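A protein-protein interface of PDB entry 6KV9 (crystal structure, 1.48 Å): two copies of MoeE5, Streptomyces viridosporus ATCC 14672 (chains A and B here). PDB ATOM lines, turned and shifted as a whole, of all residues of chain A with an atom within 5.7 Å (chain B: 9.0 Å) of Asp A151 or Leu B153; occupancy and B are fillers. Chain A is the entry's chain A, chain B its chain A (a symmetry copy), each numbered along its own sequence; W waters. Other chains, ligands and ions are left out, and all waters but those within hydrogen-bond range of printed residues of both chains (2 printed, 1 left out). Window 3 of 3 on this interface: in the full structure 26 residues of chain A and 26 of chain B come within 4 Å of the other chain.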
ATOM      1  N   TYR A 141      19.194   2.181  -0.924  1.00  0.00           N
ATOM      2  CA  TYR A 141      17.764   1.869  -0.854  1.00  0.00           C
ATOM      3  C   TYR A 141      16.895   2.987  -1.374  1.00  0.00           C
ATOM      4  O   TYR A 141      15.736   2.739  -1.737  1.00  0.00           O
ATOM      5  CB  TYR A 141      17.369   1.537   0.584  1.00  0.00           C
ATOM      6  CG  TYR A 141      17.991   0.270   1.077  1.00  0.00           C
ATOM      7  CD1 TYR A 141      17.600  -0.950   0.535  1.00  0.00           C
ATOM      8  CD2 TYR A 141      18.971   0.244   2.067  1.00  0.00           C
ATOM      9  CE1 TYR A 141      18.159  -2.123   0.978  1.00  0.00           C
ATOM     10  CE2 TYR A 141      19.511  -0.938   2.554  1.00  0.00           C
ATOM     11  CZ  TYR A 141      19.120  -2.137   1.969  1.00  0.00           C
ATOM     12  OH  TYR A 141      19.656  -3.320   2.392  1.00  0.00           O
ATOM     13  N   SER A 149      15.353  -3.745   3.888  1.00  0.00           N
ATOM     14  CA  SER A 149      15.891  -5.091   3.940  1.00  0.00           C
ATOM     15  C   SER A 149      16.760  -5.387   2.724  1.00  0.00           C
ATOM     16  O   SER A 149      16.539  -4.834   1.645  1.00  0.00           O
ATOM     17  CB  SER A 149      14.724  -6.078   3.942  1.00  0.00           C
ATOM     18  OG  SER A 149      13.971  -5.897   5.116  1.00  0.00           O
ATOM     19  N   GLU A 150      17.731  -6.257   2.934  1.00  0.00           N
ATOM     20  CA  GLU A 150      18.673  -6.594   1.869  1.00  0.00           C
ATOM     21  C   GLU A 150      17.989  -7.270   0.691  1.00  0.00           C
ATOM     22  O   GLU A 150      18.599  -7.319  -0.385  1.00  0.00           O
ATOM     23  CB  GLU A 150      19.821  -7.467   2.374  1.00  0.00           C
ATOM     24  CG  GLU A 150      20.673  -6.828   3.506  1.00  0.00           C
ATOM     25  CD  GLU A 150      20.123  -7.098   4.915  1.00  0.00           C
ATOM     26  OE1 GLU A 150      20.926  -6.974   5.835  1.00  0.00           O
ATOM     27  OE2 GLU A 150      18.909  -7.382   5.083  1.00  0.00           O
ATOM     28  N   ASP A 151      16.754  -7.729   0.831  1.00  0.00           N
ATOM     29  CA  ASP A 151      16.073  -8.225  -0.356  1.00  0.00           C
ATOM     30  C   ASP A 151      15.240  -7.185  -1.069  1.00  0.00           C
ATOM     31  O   ASP A 151      14.552  -7.523  -2.048  1.00  0.00           O
ATOM     32  CB  ASP A 151      15.292  -9.521  -0.075  1.00  0.00           C
ATOM     33  CG  ASP A 151      14.313  -9.365   1.013  1.00  0.00           C
ATOM     34  OD1 ASP A 151      14.285  -8.289   1.626  1.00  0.00           O
ATOM     35  OD2 ASP A 151      13.558 -10.326   1.284  1.00  0.00           O
ATOM     36  N   ASP A 152      15.276  -5.915  -0.636  1.00  0.00           N
ATOM     37  CA  ASP A 152      14.506  -4.876  -1.327  1.00  0.00           C
ATOM     38  C   ASP A 152      15.258  -4.381  -2.566  1.00  0.00           C
ATOM     39  O   ASP A 152      16.493  -4.316  -2.574  1.00  0.00           O
ATOM     40  CB  ASP A 152      14.274  -3.674  -0.412  1.00  0.00           C
ATOM     41  CG  ASP A 152      13.384  -4.003   0.787  1.00  0.00           C
ATOM     42  OD1 ASP A 152      12.633  -4.997   0.736  1.00  0.00           O
ATOM     43  OD2 ASP A 152      13.445  -3.222   1.775  1.00  0.00           O
ATOM     44  N   LEU A 153      14.519  -4.061  -3.613  1.00  0.00           N
ATOM     45  CA  LEU A 153      15.179  -3.526  -4.824  1.00  0.00           C
ATOM     46  C   LEU A 153      15.852  -2.181  -4.531  1.00  0.00           C
ATOM     47  O   LEU A 153      15.192  -1.240  -4.065  1.00  0.00           O
ATOM     48  CB  LEU A 153      14.181  -3.310  -5.969  1.00  0.00           C
ATOM     49  CG  LEU A 153      13.501  -4.574  -6.484  1.00  0.00           C
ATOM     50  CD1 LEU A 153      12.425  -4.166  -7.436  1.00  0.00           C
ATOM     51  CD2 LEU A 153      14.528  -5.427  -7.197  1.00  0.00           C
ATOM     52  N   PRO A 154      17.124  -2.023  -4.860  1.00  0.00           N
ATOM     53  CA  PRO A 154      17.753  -0.691  -4.684  1.00  0.00           C
ATOM     54  C   PRO A 154      17.127   0.332  -5.602  1.00  0.00           C
ATOM     55  O   PRO A 154      16.929   0.113  -6.802  1.00  0.00           O
ATOM     56  CB  PRO A 154      19.211  -0.967  -5.068  1.00  0.00           C
ATOM     57  CG  PRO A 154      19.417  -2.442  -4.636  1.00  0.00           C
ATOM     58  CD  PRO A 154      18.125  -3.064  -5.155  1.00  0.00           C
ATOM     59  N   ARG A 169      27.883  -3.643  -6.513  1.00  0.00           N
ATOM     60  CA  ARG A 169      27.578  -4.594  -7.582  1.00  0.00           C
ATOM     61  C   ARG A 169      28.829  -5.006  -8.333  1.00  0.00           C
ATOM     62  O   ARG A 169      28.972  -6.173  -8.700  1.00  0.00           O
ATOM     63  CB  ARG A 169      26.543  -4.022  -8.543  1.00  0.00           C
ATOM     64  CG  ARG A 169      25.153  -3.749  -7.919  1.00  0.00           C
ATOM     65  CD  ARG A 169      24.431  -5.022  -7.528  1.00  0.00           C
ATOM     66  NE  ARG A 169      24.482  -5.256  -6.092  1.00  0.00           N
ATOM     67  CZ  ARG A 169      23.926  -6.294  -5.472  1.00  0.00           C
ATOM     68  NH1 ARG A 169      24.042  -6.382  -4.141  1.00  0.00           N
ATOM     69  NH2 ARG A 169      23.307  -7.258  -6.168  1.00  0.00           N
ATOM     70  N   SER B 138      19.265  -6.531 -20.394  1.00  0.00           N
ATOM     71  CA  SER B 138      19.101  -7.755 -19.623  1.00  0.00           C
ATOM     72  C   SER B 138      20.321  -8.118 -18.807  1.00  0.00           C
ATOM     73  O   SER B 138      20.222  -8.901 -17.843  1.00  0.00           O
ATOM     74  CB  SER B 138      18.705  -8.927 -20.542  1.00  0.00           C
ATOM     75  OG  SER B 138      19.810  -9.373 -21.279  1.00  0.00           O
ATOM     76  N   SER B 139      21.508  -7.564 -19.156  1.00  0.00           N
ATOM     77  CA  SER B 139      22.708  -7.836 -18.399  1.00  0.00           C
ATOM     78  C   SER B 139      22.662  -7.272 -16.981  1.00  0.00           C
ATOM     79  O   SER B 139      23.455  -7.714 -16.131  1.00  0.00           O
ATOM     80  CB  SER B 139      23.959  -7.292 -19.098  1.00  0.00           C
ATOM     81  OG  SER B 139      23.928  -5.931 -19.134  1.00  0.00           O
ATOM     82  N   VAL B 140      21.670  -6.430 -16.658  1.00  0.00           N
ATOM     83  CA  VAL B 140      21.540  -6.057 -15.237  1.00  0.00           C
ATOM     84  C   VAL B 140      21.121  -7.222 -14.358  1.00  0.00           C
ATOM     85  O   VAL B 140      21.430  -7.241 -13.149  1.00  0.00           O
ATOM     86  CB  VAL B 140      20.567  -4.860 -15.035  1.00  0.00           C
ATOM     87  CG1 VAL B 140      20.947  -3.669 -15.896  1.00  0.00           C
ATOM     88  CG2 VAL B 140      19.075  -5.263 -15.227  1.00  0.00           C
ATOM     89  N   TYR B 141      20.503  -8.267 -14.946  1.00  0.00           N
ATOM     90  CA  TYR B 141      20.072  -9.395 -14.117  1.00  0.00           C
ATOM     91  C   TYR B 141      21.211 -10.304 -13.727  1.00  0.00           C
ATOM     92  O   TYR B 141      21.088 -11.049 -12.744  1.00  0.00           O
ATOM     93  CB  TYR B 141      18.997 -10.201 -14.843  1.00  0.00           C
ATOM     94  CG  TYR B 141      17.724  -9.438 -15.022  1.00  0.00           C
ATOM     95  CD1 TYR B 141      16.944  -9.124 -13.914  1.00  0.00           C
ATOM     96  CD2 TYR B 141      17.270  -9.006 -16.266  1.00  0.00           C
ATOM     97  CE1 TYR B 141      15.771  -8.427 -14.060  1.00  0.00           C
ATOM     98  CE2 TYR B 141      16.063  -8.338 -16.432  1.00  0.00           C
ATOM     99  CZ  TYR B 141      15.324  -8.014 -15.300  1.00  0.00           C
ATOM    100  OH  TYR B 141      14.151  -7.325 -15.416  1.00  0.00           O
ATOM    101  N   GLY B 142      22.265 -10.378 -14.537  1.00  0.00           N
ATOM    102  CA  GLY B 142      23.318 -11.330 -14.222  1.00  0.00           C
ATOM    103  C   GLY B 142      22.877 -12.742 -14.587  1.00  0.00           C
ATOM    104  O   GLY B 142      22.049 -12.978 -15.485  1.00  0.00           O
ATOM    105  N   GLY B 143      23.421 -13.675 -13.836  1.00  0.00           N
ATOM    106  CA  GLY B 143      23.353 -15.073 -14.234  1.00  0.00           C
ATOM    107  C   GLY B 143      22.262 -15.879 -13.574  1.00  0.00           C
ATOM    108  O   GLY B 143      22.536 -16.742 -12.733  1.00  0.00           O
ATOM    109  N   ALA B 144      21.033 -15.641 -13.997  1.00  0.00           N
ATOM    110  CA  ALA B 144      19.848 -16.336 -13.500  1.00  0.00           C
ATOM    111  C   ALA B 144      19.408 -17.457 -14.439  1.00  0.00           C
ATOM    112  O   ALA B 144      19.471 -17.326 -15.670  1.00  0.00           O
ATOM    113  CB  ALA B 144      18.705 -15.333 -13.349  1.00  0.00           C
ATOM    114  N   MET B 148      13.657 -13.982 -16.044  1.00  0.00           N
ATOM    115  CA  MET B 148      14.180 -12.766 -15.399  1.00  0.00           C
ATOM    116  C   MET B 148      13.061 -11.733 -15.317  1.00  0.00           C
ATOM    117  O   MET B 148      12.583 -11.234 -16.333  1.00  0.00           O
ATOM    118  CB  MET B 148      15.353 -12.219 -16.203  1.00  0.00           C
ATOM    119  CG  MET B 148      16.519 -13.127 -16.156  1.00  0.00           C
ATOM    120  SD  MET B 148      17.703 -12.712 -17.499  1.00  0.00           S
ATOM    121  CE  MET B 148      19.179 -13.504 -16.931  1.00  0.00           C
ATOM    122  N   SER B 149      12.609 -11.423 -14.087  1.00  0.00           N
ATOM    123  CA  SER B 149      11.494 -10.523 -13.860  1.00  0.00           C
ATOM    124  C   SER B 149      11.964  -9.190 -13.292  1.00  0.00           C
ATOM    125  O   SER B 149      12.981  -9.128 -12.597  1.00  0.00           O
ATOM    126  CB  SER B 149      10.552 -11.168 -12.843  1.00  0.00           C
ATOM    127  OG  SER B 149      10.017 -12.346 -13.394  1.00  0.00           O
ATOM    128  N   GLU B 150      11.208  -8.154 -13.605  1.00  0.00           N
ATOM    129  CA  GLU B 150      11.571  -6.808 -13.171  1.00  0.00           C
ATOM    130  C   GLU B 150      11.559  -6.671 -11.657  1.00  0.00           C
ATOM    131  O   GLU B 150      12.140  -5.698 -11.156  1.00  0.00           O
ATOM    132  CB  GLU B 150      10.673  -5.742 -13.796  1.00  0.00           C
ATOM    133  CG  GLU B 150      10.693  -5.705 -15.350  1.00  0.00           C
ATOM    134  CD  GLU B 150       9.671  -6.651 -15.999  1.00  0.00           C
ATOM    135  OE1 GLU B 150       9.365  -6.391 -17.159  1.00  0.00           O
ATOM    136  OE2 GLU B 150       9.232  -7.647 -15.368  1.00  0.00           O
ATOM    137  N   ASP B 151      10.984  -7.611 -10.922  1.00  0.00           N
ATOM    138  CA  ASP B 151      11.128  -7.531  -9.476  1.00  0.00           C
ATOM    139  C   ASP B 151      12.307  -8.304  -8.930  1.00  0.00           C
ATOM    140  O   ASP B 151      12.475  -8.368  -7.699  1.00  0.00           O
ATOM    141  CB  ASP B 151       9.814  -7.856  -8.744  1.00  0.00           C
ATOM    142  CG  ASP B 151       9.283  -9.181  -9.102  1.00  0.00           C
ATOM    143  OD1 ASP B 151       9.865  -9.827  -9.983  1.00  0.00           O
ATOM    144  OD2 ASP B 151       8.260  -9.597  -8.514  1.00  0.00           O
ATOM    145  N   ASP B 152      13.155  -8.890  -9.789  1.00  0.00           N
ATOM    146  CA  ASP B 152      14.326  -9.618  -9.293  1.00  0.00           C
ATOM    147  C   ASP B 152      15.467  -8.649  -8.968  1.00  0.00           C
ATOM    148  O   ASP B 152      15.639  -7.625  -9.640  1.00  0.00           O
ATOM    149  CB  ASP B 152      14.838 -10.604 -10.343  1.00  0.00           C
ATOM    150  CG  ASP B 152      13.847 -11.731 -10.632  1.00  0.00           C
ATOM    151  OD1 ASP B 152      12.965 -12.000  -9.793  1.00  0.00           O
ATOM    152  OD2 ASP B 152      13.990 -12.353 -11.720  1.00  0.00           O
ATOM    153  N   LEU B 153      16.222  -8.956  -7.928  1.00  0.00           N
ATOM    154  CA  LEU B 153      17.372  -8.090  -7.593  1.00  0.00           C
ATOM    155  C   LEU B 153      18.416  -8.107  -8.715  1.00  0.00           C
ATOM    156  O   LEU B 153      18.904  -9.180  -9.098  1.00  0.00           O
ATOM    157  CB  LEU B 153      18.068  -8.540  -6.302  1.00  0.00           C
ATOM    158  CG  LEU B 153      17.210  -8.467  -5.043  1.00  0.00           C
ATOM    159  CD1 LEU B 153      17.957  -9.128  -3.933  1.00  0.00           C
ATOM    160  CD2 LEU B 153      16.959  -7.013  -4.705  1.00  0.00           C
ATOM    161  N   PRO B 154      18.839  -6.953  -9.205  1.00  0.00           N
ATOM    162  CA  PRO B 154      19.929  -6.954 -10.212  1.00  0.00           C
ATOM    163  C   PRO B 154      21.220  -7.464  -9.615  1.00  0.00           C
ATOM    164  O   PRO B 154      21.650  -7.065  -8.527  1.00  0.00           O
ATOM    165  CB  PRO B 154      20.032  -5.470 -10.582  1.00  0.00           C
ATOM    166  CG  PRO B 154      18.577  -4.962 -10.411  1.00  0.00           C
ATOM    167  CD  PRO B 154      18.207  -5.626  -9.088  1.00  0.00           C
ATOM    168  N   ARG B 155      21.897  -8.329 -10.372  1.00  0.00           N
ATOM    169  CA  ARG B 155      23.143  -8.946  -9.914  1.00  0.00           C
ATOM    170  C   ARG B 155      24.083  -9.064 -11.111  1.00  0.00           C
ATOM    171  O   ARG B 155      24.484 -10.170 -11.502  1.00  0.00           O
ATOM    172  CB  ARG B 155      22.866 -10.332  -9.290  1.00  0.00           C
ATOM    173  CG  ARG B 155      21.991 -10.279  -8.010  1.00  0.00           C
ATOM    174  CD  ARG B 155      21.541 -11.684  -7.590  1.00  0.00           C
ATOM    175  NE  ARG B 155      20.903 -11.603  -6.275  1.00  0.00           N
ATOM    176  CZ  ARG B 155      20.355 -12.624  -5.619  1.00  0.00           C
ATOM    177  NH1 ARG B 155      20.355 -13.852  -6.143  1.00  0.00           N
ATOM    178  NH2 ARG B 155      19.808 -12.410  -4.422  1.00  0.00           N
ATOM    179  N   PRO B 156      24.418  -7.939 -11.759  1.00  0.00           N
ATOM    180  CA  PRO B 156      25.220  -8.034 -13.004  1.00  0.00           C
ATOM    181  C   PRO B 156      26.547  -8.735 -12.800  1.00  0.00           C
ATOM    182  O   PRO B 156      27.212  -8.609 -11.770  1.00  0.00           O
ATOM    183  CB  PRO B 156      25.424  -6.570 -13.431  1.00  0.00           C
ATOM    184  CG  PRO B 156      25.152  -5.770 -12.167  1.00  0.00           C
ATOM    185  CD  PRO B 156      24.119  -6.539 -11.368  1.00  0.00           C
ATOM    186  N   LEU B 165      23.010  -0.795 -15.314  1.00  0.00           N
ATOM    187  CA  LEU B 165      22.257  -0.630 -14.058  1.00  0.00           C
ATOM    188  C   LEU B 165      22.410   0.775 -13.502  1.00  0.00           C
ATOM    189  O   LEU B 165      21.419   1.396 -13.067  1.00  0.00           O
ATOM    190  CB  LEU B 165      22.736  -1.666 -13.045  1.00  0.00           C
ATOM    191  CG  LEU B 165      22.050  -1.582 -11.643  1.00  0.00           C
ATOM    192  CD1 LEU B 165      20.511  -1.836 -11.757  1.00  0.00           C
ATOM    193  CD2 LEU B 165      22.698  -2.595 -10.737  1.00  0.00           C
ATOM    194  N   ARG B 188      14.578  -2.699 -20.447  1.00  0.00           N
ATOM    195  CA  ARG B 188      15.667  -3.695 -20.409  1.00  0.00           C
ATOM    196  C   ARG B 188      15.507  -4.583 -21.630  1.00  0.00           C
ATOM    197  O   ARG B 188      14.753  -5.561 -21.616  1.00  0.00           O
ATOM    198  CB  ARG B 188      15.641  -4.518 -19.114  1.00  0.00           C
ATOM    199  CG  ARG B 188      15.903  -3.616 -17.874  1.00  0.00           C
ATOM    200  CD  ARG B 188      15.618  -4.371 -16.578  1.00  0.00           C
ATOM    201  NE  ARG B 188      16.029  -3.513 -15.441  1.00  0.00           N
ATOM    202  CZ  ARG B 188      15.868  -3.866 -14.164  1.00  0.00           C
ATOM    203  NH1 ARG B 188      15.251  -5.036 -13.864  1.00  0.00           N
ATOM    204  NH2 ARG B 188      16.323  -3.067 -13.181  1.00  0.00           N
HETATM  205  O   HOH W   1      26.598  -7.614  -9.252  1.00  0.00           O
HETATM  206  O   HOH W   2      20.632  -5.109  -6.700  1.00  0.00           O
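Hydrophobic or aromatic side chains of chain B within 4 Å of the printed part of chain A: Leu B153 and Leu B165. Hydrophobic or aromatic side chains of chain A within 4 Å of the printed part of chain B: Leu A153. Along chain A the printed residues that touch a printed residue of chain B span positions 151 to 169. Among the printed residues, no Asp or Glu carboxylate lies within 4 Å of a Lys or Arg side-chain nitrogen of the other chain.
Asp A151 touches Leu B153, and with the chains exchanged Leu A153 touches Asp B151. Asp A152 touches Leu B153, and with the chains exchanged Leu A153 touches Asp B152. Leu B153 touches its own counterpart, Leu A153. Positions printed for both chains: 141, 149, 150, 151, 152, 153 and 154.
Water W1 bridges O of Pro B156 and O of Arg A169. Water W2 lies within hydrogen-bond range of O of Pro B154 and NH2 of Arg A169.
Among the printed residues, pairs that only touch across the chains: Asp A152 with Leu B153, Leu A153 with Asp B152, Asp A151 with Leu B153, Leu A153 with Asp B151, Arg A169 with Arg B155, Leu A153 with Leu B153 and Arg A169 with Leu B165.
The backbone carbonyl oxygen (O) of Pro B154 sits at hydrogen-bond distance from the guanidinium group (NH2) of Arg A169 (2.9 Å).
Of chain B, only Leu B153 (3.6 Å) comes within 4 Å of Asp A151. Printed residues of chain A within 4 Å of Pro B154: Arg A169 (2.9 Å). Printed residues of chain A within 4 Å of Leu B165: Arg A169 (3.9 Å). Of the printed residues of chain A, Arg B155 touches Arg A169. Printed residues of chain A within 4 Å of Asp B151: Leu A153 (3.6 Å). Printed residues of chain B within 4 Å of Leu A153: Asp B151, Asp B152 and Leu B153. Gly B142 touches none of the printed residues of chain A. Tyr A141 touches none of the printed residues of chain B. The nearest residue of chain B that does not touch Asp A151 is Asp B151 (6.1 Å).
The side-chain carboxylate (OD2) of Asp A152 sits at hydrogen-bond distance from the backbone NH (N) of Ser A149. The backbone carbonyl oxygen (O) of Val B140 sits at hydrogen-bond distance from the backbone NH (N) of Arg B155, 3.0 Å away. OD2 of Asp B152 is in hydrogen-bond range of N of Ser B149, at 2.9 Å.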
